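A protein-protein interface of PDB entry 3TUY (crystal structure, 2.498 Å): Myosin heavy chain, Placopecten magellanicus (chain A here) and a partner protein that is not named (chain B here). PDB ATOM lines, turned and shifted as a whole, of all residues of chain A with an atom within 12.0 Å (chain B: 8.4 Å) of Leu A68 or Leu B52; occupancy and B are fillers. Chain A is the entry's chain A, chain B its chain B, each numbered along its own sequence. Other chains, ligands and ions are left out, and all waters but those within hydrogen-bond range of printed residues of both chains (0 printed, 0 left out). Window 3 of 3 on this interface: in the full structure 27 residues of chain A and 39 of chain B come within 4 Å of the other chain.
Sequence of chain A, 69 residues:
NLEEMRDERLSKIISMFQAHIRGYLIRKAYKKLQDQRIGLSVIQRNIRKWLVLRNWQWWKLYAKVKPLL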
ATOM      1  N   GLN A  57      -1.032   0.848   2.658  1.00  0.00           N
ATOM      2  CA  GLN A  57      -0.201   0.465   1.516  1.00  0.00           C
ATOM      3  C   GLN A  57      -0.390   1.349   0.273  1.00  0.00           C
ATOM      4  O   GLN A  57       0.578   1.672  -0.386  1.00  0.00           O
ATOM      5  CB  GLN A  57      -0.386  -1.019   1.175  1.00  0.00           C
ATOM      6  CG  GLN A  57       0.675  -1.953   1.752  1.00  0.00           C
ATOM      7  CD  GLN A  57       2.040  -1.791   1.083  1.00  0.00           C
ATOM      8  OE1 GLN A  57       2.209  -0.968   0.177  1.00  0.00           O
ATOM      9  NE2 GLN A  57       3.018  -2.573   1.534  1.00  0.00           N
ATOM     10  N   TRP A  58      -1.623   1.746  -0.034  1.00  0.00           N
ATOM     11  CA  TRP A  58      -1.855   2.693  -1.124  1.00  0.00           C
ATOM     12  C   TRP A  58      -1.036   3.954  -0.986  1.00  0.00           C
ATOM     13  O   TRP A  58      -0.497   4.445  -1.973  1.00  0.00           O
ATOM     14  CB  TRP A  58      -3.331   3.065  -1.274  1.00  0.00           C
ATOM     15  CG  TRP A  58      -4.077   2.069  -2.081  1.00  0.00           C
ATOM     16  CD1 TRP A  58      -5.003   1.196  -1.625  1.00  0.00           C
ATOM     17  CD2 TRP A  58      -3.945   1.817  -3.482  1.00  0.00           C
ATOM     18  NE1 TRP A  58      -5.477   0.430  -2.643  1.00  0.00           N
ATOM     19  CE2 TRP A  58      -4.840   0.780  -3.799  1.00  0.00           C
ATOM     20  CE3 TRP A  58      -3.164   2.374  -4.504  1.00  0.00           C
ATOM     21  CZ2 TRP A  58      -4.981   0.274  -5.094  1.00  0.00           C
ATOM     22  CZ3 TRP A  58      -3.295   1.874  -5.784  1.00  0.00           C
ATOM     23  CH2 TRP A  58      -4.199   0.830  -6.072  1.00  0.00           C
ATOM     24  N   TRP A  59      -0.959   4.490   0.233  1.00  0.00           N
ATOM     25  CA  TRP A  59      -0.196   5.711   0.454  1.00  0.00           C
ATOM     26  C   TRP A  59       1.287   5.455   0.278  1.00  0.00           C
ATOM     27  O   TRP A  59       1.981   6.242  -0.369  1.00  0.00           O
ATOM     28  CB  TRP A  59      -0.441   6.321   1.827  1.00  0.00           C
ATOM     29  CG  TRP A  59       0.712   7.210   2.271  1.00  0.00           C
ATOM     30  CD1 TRP A  59       1.637   6.939   3.258  1.00  0.00           C
ATOM     31  CD2 TRP A  59       1.070   8.494   1.741  1.00  0.00           C
ATOM     32  NE1 TRP A  59       2.518   7.980   3.386  1.00  0.00           N
ATOM     33  CE2 TRP A  59       2.200   8.945   2.466  1.00  0.00           C
ATOM     34  CE3 TRP A  59       0.546   9.306   0.736  1.00  0.00           C
ATOM     35  CZ2 TRP A  59       2.810  10.169   2.211  1.00  0.00           C
ATOM     36  CZ3 TRP A  59       1.153  10.527   0.482  1.00  0.00           C
ATOM     37  CH2 TRP A  59       2.273  10.947   1.214  1.00  0.00           C
ATOM     38  N   LYS A  60       1.780   4.362   0.853  1.00  0.00           N
ATOM     39  CA  LYS A  60       3.195   4.039   0.684  1.00  0.00           C
ATOM     40  C   LYS A  60       3.557   4.009  -0.806  1.00  0.00           C
ATOM     41  O   LYS A  60       4.593   4.543  -1.210  1.00  0.00           O
ATOM     42  CB  LYS A  60       3.538   2.711   1.347  1.00  0.00           C
ATOM     43  CG  LYS A  60       3.856   2.796   2.816  1.00  0.00           C
ATOM     44  CD  LYS A  60       3.545   1.471   3.482  1.00  0.00           C
ATOM     45  CE  LYS A  60       4.155   1.375   4.871  1.00  0.00           C
ATOM     46  NZ  LYS A  60       3.843   0.051   5.504  1.00  0.00           N
ATOM     47  N   LEU A  61       2.696   3.397  -1.618  1.00  0.00           N
ATOM     48  CA  LEU A  61       2.875   3.418  -3.069  1.00  0.00           C
ATOM     49  C   LEU A  61       2.827   4.852  -3.601  1.00  0.00           C
ATOM     50  O   LEU A  61       3.794   5.343  -4.210  1.00  0.00           O
ATOM     51  CB  LEU A  61       1.826   2.556  -3.781  1.00  0.00           C
ATOM     52  CG  LEU A  61       1.989   2.507  -5.303  1.00  0.00           C
ATOM     53  CD1 LEU A  61       3.418   2.183  -5.611  1.00  0.00           C
ATOM     54  CD2 LEU A  61       1.066   1.511  -5.998  1.00  0.00           C
ATOM     55  N   TYR A  62       1.703   5.520  -3.365  1.00  0.00           N
ATOM     56  CA  TYR A  62       1.498   6.877  -3.850  1.00  0.00           C
ATOM     57  C   TYR A  62       2.708   7.794  -3.594  1.00  0.00           C
ATOM     58  O   TYR A  62       3.097   8.597  -4.446  1.00  0.00           O
ATOM     59  CB  TYR A  62       0.252   7.451  -3.202  1.00  0.00           C
ATOM     60  CG  TYR A  62      -0.185   8.765  -3.762  1.00  0.00           C
ATOM     61  CD1 TYR A  62      -1.150   8.835  -4.771  1.00  0.00           C
ATOM     62  CD2 TYR A  62       0.352   9.952  -3.276  1.00  0.00           C
ATOM     63  CE1 TYR A  62      -1.573  10.070  -5.282  1.00  0.00           C
ATOM     64  CE2 TYR A  62      -0.058  11.190  -3.775  1.00  0.00           C
ATOM     65  CZ  TYR A  62      -1.019  11.245  -4.775  1.00  0.00           C
ATOM     66  OH  TYR A  62      -1.413  12.479  -5.252  1.00  0.00           O
ATOM     67  N   ALA A  63       3.321   7.656  -2.429  1.00  0.00           N
ATOM     68  CA  ALA A  63       4.426   8.526  -2.066  1.00  0.00           C
ATOM     69  C   ALA A  63       5.725   8.193  -2.800  1.00  0.00           C
ATOM     70  O   ALA A  63       6.508   9.091  -3.092  1.00  0.00           O
ATOM     71  CB  ALA A  63       4.652   8.473  -0.563  1.00  0.00           C
ATOM     72  N   LYS A  64       5.965   6.912  -3.069  1.00  0.00           N
ATOM     73  CA  LYS A  64       7.112   6.510  -3.882  1.00  0.00           C
ATOM     74  C   LYS A  64       6.931   6.927  -5.348  1.00  0.00           C
ATOM     75  O   LYS A  64       7.905   7.121  -6.071  1.00  0.00           O
ATOM     76  CB  LYS A  64       7.358   4.998  -3.783  1.00  0.00           C
ATOM     77  CG  LYS A  64       8.239   4.604  -2.625  1.00  0.00           C
ATOM     78  CD  LYS A  64       8.197   3.112  -2.350  1.00  0.00           C
ATOM     79  CE  LYS A  64       9.281   2.722  -1.343  1.00  0.00           C
ATOM     80  NZ  LYS A  64       9.501   1.242  -1.237  1.00  0.00           N
ATOM     81  N   VAL A  65       5.678   7.083  -5.766  1.00  0.00           N
ATOM     82  CA  VAL A  65       5.341   7.435  -7.141  1.00  0.00           C
ATOM     83  C   VAL A  65       5.367   8.951  -7.413  1.00  0.00           C
ATOM     84  O   VAL A  65       5.582   9.382  -8.545  1.00  0.00           O
ATOM     85  CB  VAL A  65       3.963   6.814  -7.526  1.00  0.00           C
ATOM     86  CG1 VAL A  65       3.290   7.552  -8.672  1.00  0.00           C
ATOM     87  CG2 VAL A  65       4.127   5.352  -7.862  1.00  0.00           C
ATOM     88  N   LYS A  66       5.159   9.747  -6.368  1.00  0.00           N
ATOM     89  CA  LYS A  66       4.952  11.192  -6.499  1.00  0.00           C
ATOM     90  C   LYS A  66       6.208  11.980  -6.941  1.00  0.00           C
ATOM     91  O   LYS A  66       6.098  12.960  -7.679  1.00  0.00           O
ATOM     92  CB  LYS A  66       4.389  11.736  -5.181  1.00  0.00           C
ATOM     93  CG  LYS A  66       3.859  13.172  -5.185  1.00  0.00           C
ATOM     94  CD  LYS A  66       3.773  13.680  -3.727  1.00  0.00           C
ATOM     95  CE  LYS A  66       2.554  14.564  -3.440  1.00  0.00           C
ATOM     96  NZ  LYS A  66       2.869  16.016  -3.185  1.00  0.00           N
ATOM     97  N   PRO A  67       7.403  11.556  -6.498  1.00  0.00           N
ATOM     98  CA  PRO A  67       8.663  12.185  -6.927  1.00  0.00           C
ATOM     99  C   PRO A  67       9.000  11.934  -8.396  1.00  0.00           C
ATOM    100  O   PRO A  67       9.801  12.675  -8.981  1.00  0.00           O
ATOM    101  CB  PRO A  67       9.718  11.497  -6.053  1.00  0.00           C
ATOM    102  CG  PRO A  67       8.971  10.941  -4.902  1.00  0.00           C
ATOM    103  CD  PRO A  67       7.635  10.543  -5.459  1.00  0.00           C
ATOM    104  N   LEU A  68       8.423  10.879  -8.968  1.00  0.00           N
ATOM    105  CA  LEU A  68       8.571  10.593 -10.390  1.00  0.00           C
ATOM    106  C   LEU A  68       7.620  11.471 -11.190  1.00  0.00           C
ATOM    107  O   LEU A  68       7.712  11.527 -12.409  1.00  0.00           O
ATOM    108  CB  LEU A  68       8.246   9.124 -10.655  1.00  0.00           C
ATOM    109  CG  LEU A  68       8.899   8.132  -9.694  1.00  0.00           C
ATOM    110  CD1 LEU A  68       8.427   6.709  -9.947  1.00  0.00           C
ATOM    111  CD2 LEU A  68      10.416   8.215  -9.794  1.00  0.00           C
ATOM    112  N   LEU A  69       6.722  12.157 -10.467  1.00  0.00           N
ATOM    113  CA  LEU A  69       5.555  12.881 -11.008  1.00  0.00           C
ATOM    114  C   LEU A  69       4.288  11.995 -10.983  1.00  0.00           C
ATOM    115  O   LEU A  69       3.489  12.034 -10.036  1.00  0.00           O
ATOM    116  CB  LEU A  69       5.806  13.405 -12.427  1.00  0.00           C
ATOM    117  CG  LEU A  69       6.734  14.588 -12.652  1.00  0.00           C
ATOM    118  CD1 LEU A  69       5.916  15.856 -12.943  1.00  0.00           C
ATOM    119  CD2 LEU A  69       7.676  14.766 -11.473  1.00  0.00           C
ATOM    120  N   GLU B  27      -2.072  12.194 -12.426  1.00  0.00           N
ATOM    121  CA  GLU B  27      -0.741  11.839 -12.922  1.00  0.00           C
ATOM    122  C   GLU B  27      -0.256  10.551 -12.275  1.00  0.00           C
ATOM    123  O   GLU B  27       0.320   9.678 -12.931  1.00  0.00           O
ATOM    124  CB  GLU B  27       0.269  12.962 -12.660  1.00  0.00           C
ATOM    125  CG  GLU B  27       0.621  13.812 -13.883  1.00  0.00           C
ATOM    126  CD  GLU B  27       2.015  14.460 -13.787  1.00  0.00           C
ATOM    127  OE1 GLU B  27       2.980  13.906 -14.394  1.00  0.00           O
ATOM    128  OE2 GLU B  27       2.140  15.522 -13.116  1.00  0.00           O
ATOM    129  N   ALA B  28      -0.509  10.435 -10.979  1.00  0.00           N
ATOM    130  CA  ALA B  28      -0.204   9.217 -10.253  1.00  0.00           C
ATOM    131  C   ALA B  28      -0.979   8.030 -10.831  1.00  0.00           C
ATOM    132  O   ALA B  28      -0.420   6.955 -11.047  1.00  0.00           O
ATOM    133  CB  ALA B  28      -0.523   9.398  -8.774  1.00  0.00           C
ATOM    134  N   MET B  31       0.618   6.929 -14.236  1.00  0.00           N
ATOM    135  CA  MET B  31       1.872   6.198 -14.200  1.00  0.00           C
ATOM    136  C   MET B  31       1.687   4.773 -13.712  1.00  0.00           C
ATOM    137  O   MET B  31       2.316   3.854 -14.222  1.00  0.00           O
ATOM    138  CB  MET B  31       2.892   6.900 -13.310  1.00  0.00           C
ATOM    139  CG  MET B  31       4.260   6.255 -13.379  1.00  0.00           C
ATOM    140  SD  MET B  31       5.536   7.269 -12.607  1.00  0.00           S
ATOM    141  CE  MET B  31       5.315   8.836 -13.446  1.00  0.00           C
ATOM    142  N   ILE B  32       0.855   4.592 -12.690  1.00  0.00           N
ATOM    143  CA  ILE B  32       0.601   3.252 -12.163  1.00  0.00           C
ATOM    144  C   ILE B  32      -0.122   2.413 -13.208  1.00  0.00           C
ATOM    145  O   ILE B  32       0.077   1.208 -13.276  1.00  0.00           O
ATOM    146  CB  ILE B  32      -0.242   3.278 -10.867  1.00  0.00           C
ATOM    147  CG1 ILE B  32       0.529   3.942  -9.737  1.00  0.00           C
ATOM    148  CG2 ILE B  32      -0.640   1.872 -10.460  1.00  0.00           C
ATOM    149  CD1 ILE B  32      -0.369   4.524  -8.686  1.00  0.00           C
ATOM    150  N   GLN B  34       0.227   1.141 -16.016  1.00  0.00           N
ATOM    151  CA  GLN B  34       1.173   0.785 -17.066  1.00  0.00           C
ATOM    152  C   GLN B  34       0.506   0.320 -18.383  1.00  0.00           C
ATOM    153  O   GLN B  34       0.945   0.708 -19.452  1.00  0.00           O
ATOM    154  CB  GLN B  34       2.198  -0.212 -16.524  1.00  0.00           C
ATOM    155  CG  GLN B  34       2.964   0.325 -15.284  1.00  0.00           C
ATOM    156  CD  GLN B  34       4.222   1.118 -15.652  1.00  0.00           C
ATOM    157  OE1 GLN B  34       4.348   2.311 -15.350  1.00  0.00           O
ATOM    158  NE2 GLN B  34       5.166   0.445 -16.303  1.00  0.00           N
ATOM    159  N   LEU B  45      -0.009  -3.041 -10.908  1.00  0.00           N
ATOM    160  CA  LEU B  45       0.546  -2.939  -9.569  1.00  0.00           C
ATOM    161  C   LEU B  45       1.851  -3.717  -9.441  1.00  0.00           C
ATOM    162  O   LEU B  45       2.813  -3.206  -8.877  1.00  0.00           O
ATOM    163  CB  LEU B  45      -0.476  -3.444  -8.541  1.00  0.00           C
ATOM    164  CG  LEU B  45      -1.001  -2.554  -7.413  1.00  0.00           C
ATOM    165  CD1 LEU B  45      -1.336  -1.186  -7.900  1.00  0.00           C
ATOM    166  CD2 LEU B  45      -2.227  -3.220  -6.804  1.00  0.00           C
ATOM    167  N   LYS B  46       1.894  -4.952  -9.932  1.00  0.00           N
ATOM    168  CA  LYS B  46       3.147  -5.708  -9.849  1.00  0.00           C
ATOM    169  C   LYS B  46       4.242  -4.968 -10.620  1.00  0.00           C
ATOM    170  O   LYS B  46       5.363  -4.818 -10.141  1.00  0.00           O
ATOM    171  CB  LYS B  46       2.992  -7.122 -10.398  1.00  0.00           C
ATOM    172  CG  LYS B  46       2.171  -8.069  -9.545  1.00  0.00           C
ATOM    173  CD  LYS B  46       2.170  -9.462 -10.163  1.00  0.00           C
ATOM    174  CE  LYS B  46       1.469 -10.485  -9.272  1.00  0.00           C
ATOM    175  NZ  LYS B  46       2.082 -11.849  -9.382  1.00  0.00           N
ATOM    176  N   GLU B  47       3.888  -4.478 -11.805  1.00  0.00           N
ATOM    177  CA  GLU B  47       4.800  -3.680 -12.617  1.00  0.00           C
ATOM    178  C   GLU B  47       5.311  -2.436 -11.893  1.00  0.00           C
ATOM    179  O   GLU B  47       6.523  -2.177 -11.865  1.00  0.00           O
ATOM    180  CB  GLU B  47       4.150  -3.286 -13.944  1.00  0.00           C
ATOM    181  CG  GLU B  47       5.165  -2.933 -15.015  1.00  0.00           C
ATOM    182  CD  GLU B  47       6.174  -4.064 -15.276  1.00  0.00           C
ATOM    183  OE1 GLU B  47       5.913  -5.226 -14.854  1.00  0.00           O
ATOM    184  OE2 GLU B  47       7.230  -3.785 -15.901  1.00  0.00           O
ATOM    185  N   MET B  48       4.400  -1.663 -11.311  1.00  0.00           N
ATOM    186  CA  MET B  48       4.802  -0.448 -10.631  1.00  0.00           C
ATOM    187  C   MET B  48       5.661  -0.739  -9.412  1.00  0.00           C
ATOM    188  O   MET B  48       6.667  -0.083  -9.195  1.00  0.00           O
ATOM    189  CB  MET B  48       3.596   0.375 -10.219  1.00  0.00           C
ATOM    190  CG  MET B  48       3.984   1.779  -9.764  1.00  0.00           C
ATOM    191  SD  MET B  48       4.582   2.840 -11.118  1.00  0.00           S
ATOM    192  CE  MET B  48       6.268   3.213 -10.632  1.00  0.00           C
ATOM    193  N   PHE B  49       5.262  -1.722  -8.617  1.00  0.00           N
ATOM    194  CA  PHE B  49       6.011  -2.051  -7.410  1.00  0.00           C
ATOM    195  C   PHE B  49       7.411  -2.530  -7.729  1.00  0.00           C
ATOM    196  O   PHE B  49       8.391  -2.082  -7.117  1.00  0.00           O
ATOM    197  CB  PHE B  49       5.273  -3.076  -6.547  1.00  0.00           C
ATOM    198  CG  PHE B  49       4.390  -2.443  -5.502  1.00  0.00           C
ATOM    199  CD1 PHE B  49       4.945  -1.644  -4.507  1.00  0.00           C
ATOM    200  CD2 PHE B  49       3.013  -2.616  -5.528  1.00  0.00           C
ATOM    201  CE1 PHE B  49       4.151  -1.053  -3.563  1.00  0.00           C
ATOM    202  CE2 PHE B  49       2.217  -2.027  -4.589  1.00  0.00           C
ATOM    203  CZ  PHE B  49       2.780  -1.245  -3.601  1.00  0.00           C
ATOM    204  N   SER B  50       7.507  -3.428  -8.707  1.00  0.00           N
ATOM    205  CA  SER B  50       8.806  -3.947  -9.111  1.00  0.00           C
ATOM    206  C   SER B  50       9.747  -2.878  -9.678  1.00  0.00           C
ATOM    207  O   SER B  50      10.966  -3.046  -9.622  1.00  0.00           O
ATOM    208  CB  SER B  50       8.661  -5.133 -10.072  1.00  0.00           C
ATOM    209  OG  SER B  50       7.881  -4.816 -11.207  1.00  0.00           O
ATOM    210  N   SER B  51       9.187  -1.786 -10.203  1.00  0.00           N
ATOM    211  CA  SER B  51       9.997  -0.678 -10.719  1.00  0.00           C
ATOM    212  C   SER B  51      10.571   0.159  -9.595  1.00  0.00           C
ATOM    213  O   SER B  51      11.457   0.974  -9.815  1.00  0.00           O
ATOM    214  CB  SER B  51       9.168   0.235 -11.628  1.00  0.00           C
ATOM    215  OG  SER B  51       8.764  -0.429 -12.816  1.00  0.00           O
ATOM    216  N   LEU B  52      10.057  -0.038  -8.385  1.00  0.00           N
ATOM    217  CA  LEU B  52      10.403   0.816  -7.244  1.00  0.00           C
ATOM    218  C   LEU B  52      11.197   0.088  -6.151  1.00  0.00           C
ATOM    219  O   LEU B  52      11.824   0.732  -5.306  1.00  0.00           O
ATOM    220  CB  LEU B  52       9.124   1.375  -6.624  1.00  0.00           C
ATOM    221  CG  LEU B  52       8.622   2.794  -6.890  1.00  0.00           C
ATOM    222  CD1 LEU B  52       9.537   3.610  -7.776  1.00  0.00           C
ATOM    223  CD2 LEU B  52       7.206   2.755  -7.432  1.00  0.00           C
ATOM    224  N   GLY B  53      11.153  -1.243  -6.151  1.00  0.00           N
ATOM    225  CA  GLY B  53      11.813  -2.017  -5.110  1.00  0.00           C
ATOM    226  C   GLY B  53      11.188  -3.385  -4.871  1.00  0.00           C
ATOM    227  O   GLY B  53      10.832  -4.087  -5.820  1.00  0.00           O
ATOM    228  N   ARG B  54      11.063  -3.772  -3.601  1.00  0.00           N
ATOM    229  CA  ARG B  54      10.480  -5.068  -3.254  1.00  0.00           C
ATOM    230  C   ARG B  54       9.031  -5.090  -3.697  1.00  0.00           C
ATOM    231  O   ARG B  54       8.290  -4.127  -3.483  1.00  0.00           O
ATOM    232  CB  ARG B  54      10.620  -5.365  -1.748  1.00  0.00           C
ATOM    233  CG  ARG B  54       9.356  -5.861  -1.017  1.00  0.00           C
ATOM    234  CD  ARG B  54       9.006  -4.907   0.147  1.00  0.00           C
ATOM    235  NE  ARG B  54       8.336  -5.553   1.280  1.00  0.00           N
ATOM    236  CZ  ARG B  54       8.160  -4.979   2.473  1.00  0.00           C
ATOM    237  NH1 ARG B  54       8.607  -3.744   2.697  1.00  0.00           N
ATOM    238  NH2 ARG B  54       7.543  -5.640   3.449  1.00  0.00           N
ATOM    239  N   THR B  55       8.635  -6.174  -4.347  1.00  0.00           N
ATOM    240  CA  THR B  55       7.270  -6.290  -4.820  1.00  0.00           C
ATOM    241  C   THR B  55       6.446  -7.166  -3.872  1.00  0.00           C
ATOM    242  O   THR B  55       6.841  -8.286  -3.536  1.00  0.00           O
ATOM    243  CB  THR B  55       7.238  -6.820  -6.259  1.00  0.00           C
ATOM    244  OG1 THR B  55       6.595  -8.098  -6.291  1.00  0.00           O
ATOM    245  CG2 THR B  55       8.649  -6.958  -6.787  1.00  0.00           C
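O of Met B31 lies close to OE1 of Gln B34 (2.8 Å).
Phe B49 touches Gln A57. CH2 of Trp A58 touches CD1 of Leu B45, at 3.95 Å. CD1 of Leu A61 touches CE1 of Phe B49, at 3.9 Å. Tyr A62 touches Ala B28. O of Leu A68 touches CE of Met B31, at 3.7 Å. Leu B52 touches Leu A68 (CD1 to CD1, 3.9 Å). OE1 of Glu B27 touches CB of Leu A69, 3.5 Å away.
Of the printed residues of chain B, Leu A61 touches Phe B49. No residue of chain B comes within 4 Å of Pro A67. Leu A68 touches just these residues of chain B: Met B31 (3.7 Å) and Leu B52 (3.9 Å). Printed residues of chain A within 4 Å of Leu B45: Trp A58. Lys B46 touches none of the printed residues of chain A. Glu B47 touches none of the printed residues of chain A. Met B48 touches none of the printed residues of chain A. Phe B49 touches two residues of chain A. No residue of chain A comes within 4 Å of Ser B50. No residue of chain A comes within 4 Å of Ser B51. Of the printed residues of chain A, Leu B52 touches Leu A68. No residue of chain A comes within 4 Å of Gly B53. The nearest printed residue of chain A that does not touch Leu B52 is Lys A64 (4.01 Å). The nearest printed residue of chain A that does not touch Glu B27 is Val A65 (5.6 Å).
Of the 16 printed residues of chain B, 6 touch a printed residue of chain A. Hydrophobic or aromatic side chains of chain B within 4 Å of the printed part of chain A: Ala B28, Met B31, Leu B45, Phe B49 and Leu B52. Of the 13 printed residues of chain A, 6 touch a printed residue of chain B. Hydrophobic or aromatic side chains of chain A within 4 Å of the printed part of chain B: Trp A58, Leu A61, Tyr A62, Leu A68 and Leu A69. Among the printed residues, 7 pairs touch across the chains. Among the printed residues, no Asp or Glu carboxylate lies within 4 Å of a Lys or Arg side-chain nitrogen of the other chain.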
